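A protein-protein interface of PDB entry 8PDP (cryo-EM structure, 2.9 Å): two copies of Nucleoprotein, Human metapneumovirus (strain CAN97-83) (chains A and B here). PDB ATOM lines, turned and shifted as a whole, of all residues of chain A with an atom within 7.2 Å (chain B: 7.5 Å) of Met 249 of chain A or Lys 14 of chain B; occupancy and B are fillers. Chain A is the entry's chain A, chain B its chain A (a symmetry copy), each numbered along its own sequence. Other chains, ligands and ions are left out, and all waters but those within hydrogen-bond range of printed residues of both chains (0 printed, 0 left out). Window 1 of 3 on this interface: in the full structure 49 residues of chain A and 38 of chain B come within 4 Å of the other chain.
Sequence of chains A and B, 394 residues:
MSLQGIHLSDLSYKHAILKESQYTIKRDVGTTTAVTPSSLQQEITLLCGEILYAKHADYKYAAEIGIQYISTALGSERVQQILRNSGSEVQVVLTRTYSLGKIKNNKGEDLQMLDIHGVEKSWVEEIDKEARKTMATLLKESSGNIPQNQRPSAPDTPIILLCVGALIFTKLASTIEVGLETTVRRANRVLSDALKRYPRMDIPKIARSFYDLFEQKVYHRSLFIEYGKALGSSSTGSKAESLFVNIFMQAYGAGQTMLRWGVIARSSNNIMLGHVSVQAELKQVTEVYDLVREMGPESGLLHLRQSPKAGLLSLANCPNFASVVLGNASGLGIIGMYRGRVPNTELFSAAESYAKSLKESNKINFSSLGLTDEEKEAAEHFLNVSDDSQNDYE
The backbone carbonyl oxygen of Lys 229 of chain A lies close to the backbone carbonyl oxygen of Leu 18 of chain B.
NH2 of Arg 260 of chain A lies within salt-bridge range of OD1 of Asp 10 of chain B.
Met 249 of chain A touches just these residues of chain B: Lys 14 and Leu 18.
Printed residues of chain B within 4 Å of Pro 297 of chain A: Tyr 13 (3.6 Å), Ala 16 (3.96 Å) and Ile 17 (3.9 Å).
Lys 14 of chain B touches just these residues of chain A: Met 249 and Tyr 252.
Of the printed residues of chain A, Pro 308 of chain B touches Val 245.
Of the printed residues of chain A, Lys 309 of chain B touches Gly 232.
The nearest residue of chain A that does not touch Lys 14 of chain B is Pro 297 of chain A (5.5 Å).
The nearest printed residue of chain A that does not touch Leu 18 of chain B is Phe 248 of chain A (4.7 Å).
Printed residues of chain B that touch a printed residue of chain A: Asp 10, Tyr 13, Lys 14, Ala 16, Ile 17, Leu 18, Pro 308, Lys 309 and Gly 311.
Printed residues of chain A that touch a printed residue of chain B: Gly 228, Lys 229, Gly 232, Val 245, Asn 246, Met 249, Tyr 252, Arg 260, Pro 297 and Leu 301.
Hydrophobic or aromatic side chains of chain A within 4 Å of the printed part of chain B: Val 245, Met 249, Tyr 252, Pro 297 and Leu 301.
Among the printed residues, Asp or Glu carboxylates within 4 Å of a Lys or Arg side-chain nitrogen of the other chain: Arg 260 of chain A with Asp 10 of chain B.
No position is printed for both chains.
Of the 17 pairs that touch across the chains among the printed residues, none has its exchanged pair printed and touching as well.
Gly 228 of chain A touches Leu 18 of chain B.
CG of Lys 229 of chain A touches O of Ile 17 of chain B (3.5 Å).
CB of Lys 309 of chain B touches O of Gly 232 of chain A, 3.3 Å away.
CG2 of Val 245 of chain A touches CB of Pro 308 of chain B, 3.4 Å away.
CA of Gly 311 of chain B touches OD1 of Asn 246 of chain A (3.9 Å).
Met 249 of chain A touches Lys 14 of chain B.
CD2 of Leu 18 of chain B touches CE of Met 249 of chain A, 2.8 Å away.
Lys 14 of chain B touches Tyr 252 of chain A (CG to CG, 3.9 Å).
CA of Pro 297 of chain A touches CG of Tyr 13 of chain B, 3.6 Å away.
Pro 297 of chain A touches Ala 16 of chain B (CB to CB, 3.96 Å).
OH of Tyr 252 of chain A lies within hydrogen-bond range of O of Pro 297 of chain A, 2.6 Å away.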
ATOM      1  N   THR A 170       2.670  13.138  22.634  1.00  0.00           N
ATOM      2  CA  THR A 170       3.445  13.723  21.541  1.00  0.00           C
ATOM      3  C   THR A 170       4.806  13.056  21.383  1.00  0.00           C
ATOM      4  O   THR A 170       5.357  13.030  20.278  1.00  0.00           O
ATOM      5  CB  THR A 170       3.633  15.224  21.758  1.00  0.00           C
ATOM      6  OG1 THR A 170       4.191  15.457  23.055  1.00  0.00           O
ATOM      7  CG2 THR A 170       2.316  15.945  21.650  1.00  0.00           C
ATOM      8  N   GLY A 228      -9.321  12.710  20.707  1.00  0.00           N
ATOM      9  CA  GLY A 228      -8.854  13.904  20.024  1.00  0.00           C
ATOM     10  C   GLY A 228      -9.670  14.223  18.788  1.00  0.00           C
ATOM     11  O   GLY A 228      -9.976  15.386  18.514  1.00  0.00           O
ATOM     12  N   LYS A 229     -10.023  13.193  18.017  1.00  0.00           N
ATOM     13  CA  LYS A 229     -10.831  13.384  16.817  1.00  0.00           C
ATOM     14  C   LYS A 229     -12.225  13.892  17.154  1.00  0.00           C
ATOM     15  O   LYS A 229     -12.774  14.741  16.445  1.00  0.00           O
ATOM     16  CB  LYS A 229     -10.930  12.072  16.043  1.00  0.00           C
ATOM     17  CG  LYS A 229      -9.694  11.690  15.272  1.00  0.00           C
ATOM     18  CD  LYS A 229      -9.952  10.418  14.494  1.00  0.00           C
ATOM     19  CE  LYS A 229      -8.779  10.053  13.616  1.00  0.00           C
ATOM     20  NZ  LYS A 229      -9.090   8.869  12.771  1.00  0.00           N
ATOM     21  N   GLY A 232     -11.915  17.578  18.328  1.00  0.00           N
ATOM     22  CA  GLY A 232     -11.677  18.505  17.242  1.00  0.00           C
ATOM     23  C   GLY A 232     -12.867  18.730  16.341  1.00  0.00           C
ATOM     24  O   GLY A 232     -12.854  19.688  15.564  1.00  0.00           O
ATOM     25  N   LEU A 243      -6.614  23.660  24.014  1.00  0.00           N
ATOM     26  CA  LEU A 243      -5.220  23.329  24.291  1.00  0.00           C
ATOM     27  C   LEU A 243      -4.941  21.853  24.038  1.00  0.00           C
ATOM     28  O   LEU A 243      -3.907  21.494  23.457  1.00  0.00           O
ATOM     29  CB  LEU A 243      -4.883  23.692  25.734  1.00  0.00           C
ATOM     30  CG  LEU A 243      -3.493  23.300  26.217  1.00  0.00           C
ATOM     31  CD1 LEU A 243      -2.465  23.816  25.240  1.00  0.00           C
ATOM     32  CD2 LEU A 243      -3.246  23.839  27.602  1.00  0.00           C
ATOM     33  N   PHE A 244      -5.848  20.983  24.484  1.00  0.00           N
ATOM     34  CA  PHE A 244      -5.686  19.554  24.255  1.00  0.00           C
ATOM     35  C   PHE A 244      -5.633  19.241  22.771  1.00  0.00           C
ATOM     36  O   PHE A 244      -4.785  18.463  22.330  1.00  0.00           O
ATOM     37  CB  PHE A 244      -6.822  18.778  24.918  1.00  0.00           C
ATOM     38  CG  PHE A 244      -6.747  17.292  24.709  1.00  0.00           C
ATOM     39  CD1 PHE A 244      -7.286  16.705  23.576  1.00  0.00           C
ATOM     40  CD2 PHE A 244      -6.150  16.479  25.648  1.00  0.00           C
ATOM     41  CE1 PHE A 244      -7.218  15.348  23.383  1.00  0.00           C
ATOM     42  CE2 PHE A 244      -6.085  15.120  25.457  1.00  0.00           C
ATOM     43  CZ  PHE A 244      -6.619  14.556  24.323  1.00  0.00           C
ATOM     44  N   VAL A 245      -6.536  19.825  21.985  1.00  0.00           N
ATOM     45  CA  VAL A 245      -6.523  19.535  20.557  1.00  0.00           C
ATOM     46  C   VAL A 245      -5.279  20.120  19.899  1.00  0.00           C
ATOM     47  O   VAL A 245      -4.755  19.547  18.939  1.00  0.00           O
ATOM     48  CB  VAL A 245      -7.819  20.023  19.891  1.00  0.00           C
ATOM     49  CG1 VAL A 245      -7.835  19.651  18.436  1.00  0.00           C
ATOM     50  CG2 VAL A 245      -9.007  19.403  20.578  1.00  0.00           C
ATOM     51  N   ASN A 246      -4.761  21.236  20.414  1.00  0.00           N
ATOM     52  CA  ASN A 246      -3.519  21.786  19.876  1.00  0.00           C
ATOM     53  C   ASN A 246      -2.347  20.840  20.102  1.00  0.00           C
ATOM     54  O   ASN A 246      -1.574  20.558  19.179  1.00  0.00           O
ATOM     55  CB  ASN A 246      -3.235  23.149  20.502  1.00  0.00           C
ATOM     56  CG  ASN A 246      -4.085  24.248  19.914  1.00  0.00           C
ATOM     57  OD1 ASN A 246      -4.675  24.089  18.851  1.00  0.00           O
ATOM     58  ND2 ASN A 246      -4.152  25.375  20.606  1.00  0.00           N
ATOM     59  N   ILE A 247      -2.198  20.330  21.327  1.00  0.00           N
ATOM     60  CA  ILE A 247      -1.120  19.377  21.598  1.00  0.00           C
ATOM     61  C   ILE A 247      -1.328  18.092  20.804  1.00  0.00           C
ATOM     62  O   ILE A 247      -0.378  17.518  20.253  1.00  0.00           O
ATOM     63  CB  ILE A 247      -1.003  19.090  23.106  1.00  0.00           C
ATOM     64  CG1 ILE A 247      -0.990  20.381  23.915  1.00  0.00           C
ATOM     65  CG2 ILE A 247       0.258  18.318  23.396  1.00  0.00           C
ATOM     66  CD1 ILE A 247      -1.178  20.146  25.393  1.00  0.00           C
ATOM     67  N   PHE A 248      -2.576  17.631  20.719  1.00  0.00           N
ATOM     68  CA  PHE A 248      -2.889  16.423  19.968  1.00  0.00           C
ATOM     69  C   PHE A 248      -2.504  16.565  18.502  1.00  0.00           C
ATOM     70  O   PHE A 248      -1.947  15.637  17.909  1.00  0.00           O
ATOM     71  CB  PHE A 248      -4.377  16.113  20.118  1.00  0.00           C
ATOM     72  CG  PHE A 248      -4.830  14.918  19.346  1.00  0.00           C
ATOM     73  CD1 PHE A 248      -4.595  13.642  19.819  1.00  0.00           C
ATOM     74  CD2 PHE A 248      -5.501  15.069  18.149  1.00  0.00           C
ATOM     75  CE1 PHE A 248      -5.010  12.546  19.105  1.00  0.00           C
ATOM     76  CE2 PHE A 248      -5.915  13.975  17.431  1.00  0.00           C
ATOM     77  CZ  PHE A 248      -5.671  12.714  17.910  1.00  0.00           C
ATOM     78  N   MET A 249      -2.790  17.715  17.896  1.00  0.00           N
ATOM     79  CA  MET A 249      -2.365  17.937  16.521  1.00  0.00           C
ATOM     80  C   MET A 249      -0.858  18.099  16.418  1.00  0.00           C
ATOM     81  O   MET A 249      -0.280  17.819  15.365  1.00  0.00           O
ATOM     82  CB  MET A 249      -3.063  19.162  15.938  1.00  0.00           C
ATOM     83  CG  MET A 249      -4.541  18.987  15.686  1.00  0.00           C
ATOM     84  SD  MET A 249      -4.879  17.651  14.532  1.00  0.00           S
ATOM     85  CE  MET A 249      -6.276  16.881  15.326  1.00  0.00           C
ATOM     86  N   GLN A 250      -0.209  18.573  17.482  1.00  0.00           N
ATOM     87  CA  GLN A 250       1.248  18.599  17.489  1.00  0.00           C
ATOM     88  C   GLN A 250       1.839  17.201  17.534  1.00  0.00           C
ATOM     89  O   GLN A 250       2.980  17.007  17.108  1.00  0.00           O
ATOM     90  CB  GLN A 250       1.763  19.416  18.671  1.00  0.00           C
ATOM     91  CG  GLN A 250       1.703  20.905  18.439  1.00  0.00           C
ATOM     92  CD  GLN A 250       2.071  21.702  19.663  1.00  0.00           C
ATOM     93  OE1 GLN A 250       2.311  21.148  20.731  1.00  0.00           O
ATOM     94  NE2 GLN A 250       2.127  23.015  19.513  1.00  0.00           N
ATOM     95  N   ALA A 251       1.084  16.227  18.031  1.00  0.00           N
ATOM     96  CA  ALA A 251       1.531  14.840  18.062  1.00  0.00           C
ATOM     97  C   ALA A 251       1.415  14.142  16.718  1.00  0.00           C
ATOM     98  O   ALA A 251       1.871  13.004  16.601  1.00  0.00           O
ATOM     99  CB  ALA A 251       0.729  14.048  19.095  1.00  0.00           C
ATOM    100  N   TYR A 252       0.847  14.795  15.707  1.00  0.00           N
ATOM    101  CA  TYR A 252       0.354  14.112  14.518  1.00  0.00           C
ATOM    102  C   TYR A 252       1.445  13.329  13.803  1.00  0.00           C
ATOM    103  O   TYR A 252       1.442  12.098  13.846  1.00  0.00           O
ATOM    104  CB  TYR A 252      -0.281  15.120  13.559  1.00  0.00           C
ATOM    105  CG  TYR A 252      -0.729  14.534  12.243  1.00  0.00           C
ATOM    106  CD1 TYR A 252      -1.802  13.660  12.186  1.00  0.00           C
ATOM    107  CD2 TYR A 252      -0.083  14.849  11.064  1.00  0.00           C
ATOM    108  CE1 TYR A 252      -2.219  13.125  10.991  1.00  0.00           C
ATOM    109  CE2 TYR A 252      -0.489  14.314   9.869  1.00  0.00           C
ATOM    110  CZ  TYR A 252      -1.557  13.452   9.837  1.00  0.00           C
ATOM    111  OH  TYR A 252      -1.964  12.916   8.642  1.00  0.00           O
ATOM    112  N   GLY A 253       2.405  14.006  13.188  1.00  0.00           N
ATOM    113  CA  GLY A 253       3.363  13.310  12.348  1.00  0.00           C
ATOM    114  C   GLY A 253       4.476  12.607  13.098  1.00  0.00           C
ATOM    115  O   GLY A 253       5.586  12.470  12.580  1.00  0.00           O
ATOM    116  N   ARG A 260       9.167  15.045   6.918  1.00  0.00           N
ATOM    117  CA  ARG A 260       9.006  16.489   7.045  1.00  0.00           C
ATOM    118  C   ARG A 260      10.310  17.221   6.765  1.00  0.00           C
ATOM    119  O   ARG A 260      10.315  18.255   6.089  1.00  0.00           O
ATOM    120  CB  ARG A 260       8.480  16.835   8.438  1.00  0.00           C
ATOM    121  CG  ARG A 260       6.971  16.725   8.579  1.00  0.00           C
ATOM    122  CD  ARG A 260       6.510  15.298   8.776  1.00  0.00           C
ATOM    123  NE  ARG A 260       5.073  15.175   8.557  1.00  0.00           N
ATOM    124  CZ  ARG A 260       4.433  14.021   8.432  1.00  0.00           C
ATOM    125  NH1 ARG A 260       5.102  12.882   8.499  1.00  0.00           N
ATOM    126  NH2 ARG A 260       3.125  14.004   8.236  1.00  0.00           N
ATOM    127  N   PRO A 297      -4.867  10.696   5.255  1.00  0.00           N
ATOM    128  CA  PRO A 297      -4.752  11.364   6.561  1.00  0.00           C
ATOM    129  C   PRO A 297      -4.328  10.451   7.694  1.00  0.00           C
ATOM    130  O   PRO A 297      -3.651  10.912   8.619  1.00  0.00           O
ATOM    131  CB  PRO A 297      -6.164  11.923   6.794  1.00  0.00           C
ATOM    132  CG  PRO A 297      -7.026  11.308   5.754  1.00  0.00           C
ATOM    133  CD  PRO A 297      -6.151  10.980   4.604  1.00  0.00           C
ATOM    134  N   LEU A 301      -0.847   9.121  11.759  1.00  0.00           N
ATOM    135  CA  LEU A 301      -1.080   8.488  13.049  1.00  0.00           C
ATOM    136  C   LEU A 301      -0.538   7.070  13.119  1.00  0.00           C
ATOM    137  O   LEU A 301      -0.820   6.363  14.088  1.00  0.00           O
ATOM    138  CB  LEU A 301      -2.573   8.479  13.367  1.00  0.00           C
ATOM    139  CG  LEU A 301      -3.285   9.825  13.281  1.00  0.00           C
ATOM    140  CD1 LEU A 301      -4.766   9.607  13.097  1.00  0.00           C
ATOM    141  CD2 LEU A 301      -3.007  10.663  14.511  1.00  0.00           C
ATOM    142  N   SER B   9       1.433  17.742   2.656  1.00  0.00           N
ATOM    143  CA  SER B   9       0.032  18.109   2.883  1.00  0.00           C
ATOM    144  C   SER B   9      -0.455  17.666   4.265  1.00  0.00           C
ATOM    145  O   SER B   9      -1.467  16.978   4.398  1.00  0.00           O
ATOM    146  CB  SER B   9      -0.868  17.541   1.785  1.00  0.00           C
ATOM    147  OG  SER B   9      -2.230  17.801   2.067  1.00  0.00           O
ATOM    148  N   ASP B  10       0.259  18.099   5.305  1.00  0.00           N
ATOM    149  CA  ASP B  10      -0.069  17.672   6.663  1.00  0.00           C
ATOM    150  C   ASP B  10      -1.298  18.389   7.207  1.00  0.00           C
ATOM    151  O   ASP B  10      -2.062  17.805   7.982  1.00  0.00           O
ATOM    152  CB  ASP B  10       1.117  17.904   7.592  1.00  0.00           C
ATOM    153  CG  ASP B  10       2.271  16.989   7.295  1.00  0.00           C
ATOM    154  OD1 ASP B  10       2.030  15.865   6.808  1.00  0.00           O
ATOM    155  OD2 ASP B  10       3.426  17.390   7.544  1.00  0.00           O
ATOM    156  N   LEU B  11      -1.487  19.660   6.851  1.00  0.00           N
ATOM    157  CA  LEU B  11      -2.597  20.423   7.414  1.00  0.00           C
ATOM    158  C   LEU B  11      -3.940  19.919   6.900  1.00  0.00           C
ATOM    159  O   LEU B  11      -4.912  19.832   7.660  1.00  0.00           O
ATOM    160  CB  LEU B  11      -2.420  21.904   7.102  1.00  0.00           C
ATOM    161  CG  LEU B  11      -3.340  22.842   7.874  1.00  0.00           C
ATOM    162  CD1 LEU B  11      -2.911  22.919   9.319  1.00  0.00           C
ATOM    163  CD2 LEU B  11      -3.310  24.206   7.236  1.00  0.00           C
ATOM    164  N   SER B  12      -4.008  19.582   5.613  1.00  0.00           N
ATOM    165  CA  SER B  12      -5.207  18.955   5.075  1.00  0.00           C
ATOM    166  C   SER B  12      -5.490  17.635   5.775  1.00  0.00           C
ATOM    167  O   SER B  12      -6.647  17.313   6.063  1.00  0.00           O
ATOM    168  CB  SER B  12      -5.048  18.739   3.572  1.00  0.00           C
ATOM    169  OG  SER B  12      -6.256  18.287   2.993  1.00  0.00           O
ATOM    170  N   TYR B  13      -4.442  16.863   6.066  1.00  0.00           N
ATOM    171  CA  TYR B  13      -4.620  15.586   6.744  1.00  0.00           C
ATOM    172  C   TYR B  13      -5.113  15.774   8.170  1.00  0.00           C
ATOM    173  O   TYR B  13      -5.952  15.006   8.645  1.00  0.00           O
ATOM    174  CB  TYR B  13      -3.309  14.805   6.731  1.00  0.00           C
ATOM    175  CG  TYR B  13      -2.956  14.245   5.378  1.00  0.00           C
ATOM    176  CD1 TYR B  13      -3.879  14.250   4.348  1.00  0.00           C
ATOM    177  CD2 TYR B  13      -1.700  13.721   5.129  1.00  0.00           C
ATOM    178  CE1 TYR B  13      -3.566  13.745   3.112  1.00  0.00           C
ATOM    179  CE2 TYR B  13      -1.376  13.214   3.894  1.00  0.00           C
ATOM    180  CZ  TYR B  13      -2.313  13.231   2.889  1.00  0.00           C
ATOM    181  OH  TYR B  13      -2.002  12.730   1.652  1.00  0.00           O
ATOM    182  N   LYS B  14      -4.598  16.785   8.875  1.00  0.00           N
ATOM    183  CA  LYS B  14      -5.067  17.058  10.229  1.00  0.00           C
ATOM    184  C   LYS B  14      -6.521  17.511  10.232  1.00  0.00           C
ATOM    185  O   LYS B  14      -7.304  17.102  11.099  1.00  0.00           O
ATOM    186  CB  LYS B  14      -4.189  18.114  10.889  1.00  0.00           C
ATOM    187  CG  LYS B  14      -2.782  17.672  11.191  1.00  0.00           C
ATOM    188  CD  LYS B  14      -2.042  18.768  11.919  1.00  0.00           C
ATOM    189  CE  LYS B  14      -0.605  18.848  11.474  1.00  0.00           C
ATOM    190  NZ  LYS B  14      -0.053  20.202  11.718  1.00  0.00           N
ATOM    191  N   HIS B  15      -6.902  18.356   9.274  1.00  0.00           N
ATOM    192  CA  HIS B  15      -8.303  18.745   9.185  1.00  0.00           C
ATOM    193  C   HIS B  15      -9.187  17.549   8.866  1.00  0.00           C
ATOM    194  O   HIS B  15     -10.264  17.396   9.451  1.00  0.00           O
ATOM    195  CB  HIS B  15      -8.498  19.846   8.147  1.00  0.00           C
ATOM    196  CG  HIS B  15      -9.889  20.400   8.124  1.00  0.00           C
ATOM    197  ND1 HIS B  15     -10.565  20.768   9.267  1.00  0.00           N
ATOM    198  CD2 HIS B  15     -10.715  20.681   7.091  1.00  0.00           C
ATOM    199  CE1 HIS B  15     -11.756  21.234   8.937  1.00  0.00           C
ATOM    200  NE2 HIS B  15     -11.873  21.193   7.623  1.00  0.00           N
ATOM    201  N   ALA B  16      -8.750  16.684   7.949  1.00  0.00           N
ATOM    202  CA  ALA B  16      -9.530  15.496   7.620  1.00  0.00           C
ATOM    203  C   ALA B  16      -9.654  14.572   8.820  1.00  0.00           C
ATOM    204  O   ALA B  16     -10.690  13.928   9.014  1.00  0.00           O
ATOM    205  CB  ALA B  16      -8.897  14.763   6.441  1.00  0.00           C
ATOM    206  N   ILE B  17      -8.600  14.481   9.630  1.00  0.00           N
ATOM    207  CA  ILE B  17      -8.653  13.688  10.852  1.00  0.00           C
ATOM    208  C   ILE B  17      -9.696  14.259  11.804  1.00  0.00           C
ATOM    209  O   ILE B  17     -10.524  13.529  12.359  1.00  0.00           O
ATOM    210  CB  ILE B  17      -7.260  13.634  11.506  1.00  0.00           C
ATOM    211  CG1 ILE B  17      -6.358  12.661  10.756  1.00  0.00           C
ATOM    212  CG2 ILE B  17      -7.357  13.255  12.971  1.00  0.00           C
ATOM    213  CD1 ILE B  17      -6.891  11.263  10.706  1.00  0.00           C
ATOM    214  N   LEU B  18      -9.673  15.577  12.001  1.00  0.00           N
ATOM    215  CA  LEU B  18     -10.543  16.194  12.999  1.00  0.00           C
ATOM    216  C   LEU B  18     -12.006  16.154  12.572  1.00  0.00           C
ATOM    217  O   LEU B  18     -12.881  15.773  13.359  1.00  0.00           O
ATOM    218  CB  LEU B  18     -10.096  17.630  13.260  1.00  0.00           C
ATOM    219  CG  LEU B  18      -8.874  17.751  14.168  1.00  0.00           C
ATOM    220  CD1 LEU B  18      -8.649  19.189  14.597  1.00  0.00           C
ATOM    221  CD2 LEU B  18      -9.027  16.848  15.377  1.00  0.00           C
ATOM    222  N   LYS B  19     -12.296  16.541  11.329  1.00  0.00           N
ATOM    223  CA  LYS B  19     -13.685  16.676  10.902  1.00  0.00           C
ATOM    224  C   LYS B  19     -14.362  15.322  10.726  1.00  0.00           C
ATOM    225  O   LYS B  19     -15.541  15.166  11.060  1.00  0.00           O
ATOM    226  CB  LYS B  19     -13.759  17.500   9.615  1.00  0.00           C
ATOM    227  CG  LYS B  19     -13.114  16.858   8.405  1.00  0.00           C
ATOM    228  CD  LYS B  19     -13.189  17.765   7.196  1.00  0.00           C
ATOM    229  CE  LYS B  19     -12.550  17.112   5.987  1.00  0.00           C
ATOM    230  NZ  LYS B  19     -12.599  17.988   4.787  1.00  0.00           N
ATOM    231  N   GLU B  20     -13.640  14.329  10.208  1.00  0.00           N
ATOM    232  CA  GLU B  20     -14.232  13.030   9.886  1.00  0.00           C
ATOM    233  C   GLU B  20     -14.182  12.127  11.117  1.00  0.00           C
ATOM    234  O   GLU B  20     -13.374  11.202  11.223  1.00  0.00           O
ATOM    235  CB  GLU B  20     -13.524  12.405   8.692  1.00  0.00           C
ATOM    236  CG  GLU B  20     -13.577  13.263   7.440  1.00  0.00           C
ATOM    237  CD  GLU B  20     -12.474  12.939   6.456  1.00  0.00           C
ATOM    238  OE1 GLU B  20     -12.296  13.711   5.489  1.00  0.00           O
ATOM    239  OE2 GLU B  20     -11.792  11.911   6.645  1.00  0.00           O
ATOM    240  N   GLN B 284       3.216  26.407   2.974  1.00  0.00           N
ATOM    241  CA  GLN B 284       2.352  26.139   4.117  1.00  0.00           C
ATOM    242  C   GLN B 284       1.376  27.285   4.366  1.00  0.00           C
ATOM    243  O   GLN B 284       0.265  27.054   4.853  1.00  0.00           O
ATOM    244  CB  GLN B 284       3.200  25.859   5.353  1.00  0.00           C
ATOM    245  CG  GLN B 284       3.842  24.481   5.326  1.00  0.00           C
ATOM    246  CD  GLN B 284       4.322  24.019   6.684  1.00  0.00           C
ATOM    247  OE1 GLN B 284       3.725  24.342   7.711  1.00  0.00           O
ATOM    248  NE2 GLN B 284       5.411  23.259   6.698  1.00  0.00           N
ATOM    249  N   LEU B 291      -7.047  25.790   3.657  1.00  0.00           N
ATOM    250  CA  LEU B 291      -7.854  25.250   4.746  1.00  0.00           C
ATOM    251  C   LEU B 291      -9.007  26.179   5.082  1.00  0.00           C
ATOM    252  O   LEU B 291     -10.119  25.723   5.366  1.00  0.00           O
ATOM    253  CB  LEU B 291      -6.989  25.019   5.981  1.00  0.00           C
ATOM    254  CG  LEU B 291      -7.732  24.415   7.168  1.00  0.00           C
ATOM    255  CD1 LEU B 291      -8.490  23.188   6.737  1.00  0.00           C
ATOM    256  CD2 LEU B 291      -6.788  24.094   8.293  1.00  0.00           C
ATOM    257  N   PRO B 308     -12.475  23.698  19.418  1.00  0.00           N
ATOM    258  CA  PRO B 308     -11.118  23.144  19.494  1.00  0.00           C
ATOM    259  C   PRO B 308     -10.433  23.041  18.148  1.00  0.00           C
ATOM    260  O   PRO B 308      -9.199  23.030  18.097  1.00  0.00           O
ATOM    261  CB  PRO B 308     -11.343  21.763  20.120  1.00  0.00           C
ATOM    262  CG  PRO B 308     -12.654  21.872  20.811  1.00  0.00           C
ATOM    263  CD  PRO B 308     -13.473  22.757  19.945  1.00  0.00           C
ATOM    264  N   LYS B 309     -11.195  22.984  17.057  1.00  0.00           N
ATOM    265  CA  LYS B 309     -10.614  22.937  15.722  1.00  0.00           C
ATOM    266  C   LYS B 309      -9.848  24.206  15.381  1.00  0.00           C
ATOM    267  O   LYS B 309      -8.982  24.177  14.501  1.00  0.00           O
ATOM    268  CB  LYS B 309     -11.718  22.686  14.695  1.00  0.00           C
ATOM    269  CG  LYS B 309     -11.213  22.325  13.322  1.00  0.00           C
ATOM    270  CD  LYS B 309     -12.341  21.949  12.389  1.00  0.00           C
ATOM    271  CE  LYS B 309     -13.369  23.044  12.275  1.00  0.00           C
ATOM    272  NZ  LYS B 309     -14.239  22.804  11.099  1.00  0.00           N
ATOM    273  N   GLY B 311      -6.968  26.778  15.636  1.00  0.00           N
ATOM    274  CA  GLY B 311      -5.577  26.413  15.809  1.00  0.00           C
ATOM    275  C   GLY B 311      -4.988  25.734  14.597  1.00  0.00           C
ATOM    276  O   GLY B 311      -3.767  25.779  14.402  1.00  0.00           O
ATOM    277  N   LEU B 312      -5.824  25.097  13.778  1.00  0.00           N
ATOM    278  CA  LEU B 312      -5.393  24.693  12.448  1.00  0.00           C
ATOM    279  C   LEU B 312      -5.183  25.905  11.556  1.00  0.00           C
ATOM    280  O   LEU B 312      -4.350  25.867  10.645  1.00  0.00           O
ATOM    281  CB  LEU B 312      -6.420  23.749  11.829  1.00  0.00           C
ATOM    282  CG  LEU B 312      -6.590  22.363  12.449  1.00  0.00           C
ATOM    283  CD1 LEU B 312      -7.790  21.670  11.844  1.00  0.00           C
ATOM    284  CD2 LEU B 312      -5.341  21.539  12.234  1.00  0.00           C
ATOM    285  N   ASN B 317       3.595  28.688  12.680  1.00  0.00           N
ATOM    286  CA  ASN B 317       4.735  27.918  12.202  1.00  0.00           C
ATOM    287  C   ASN B 317       5.331  28.506  10.930  1.00  0.00           C
ATOM    288  O   ASN B 317       5.973  27.785  10.160  1.00  0.00           O
ATOM    289  CB  ASN B 317       4.338  26.458  11.988  1.00  0.00           C
ATOM    290  CG  ASN B 317       4.071  25.730  13.292  1.00  0.00           C
ATOM    291  OD1 ASN B 317       4.799  25.898  14.270  1.00  0.00           O
ATOM    292  ND2 ASN B 317       3.020  24.920  13.313  1.00  0.00           N
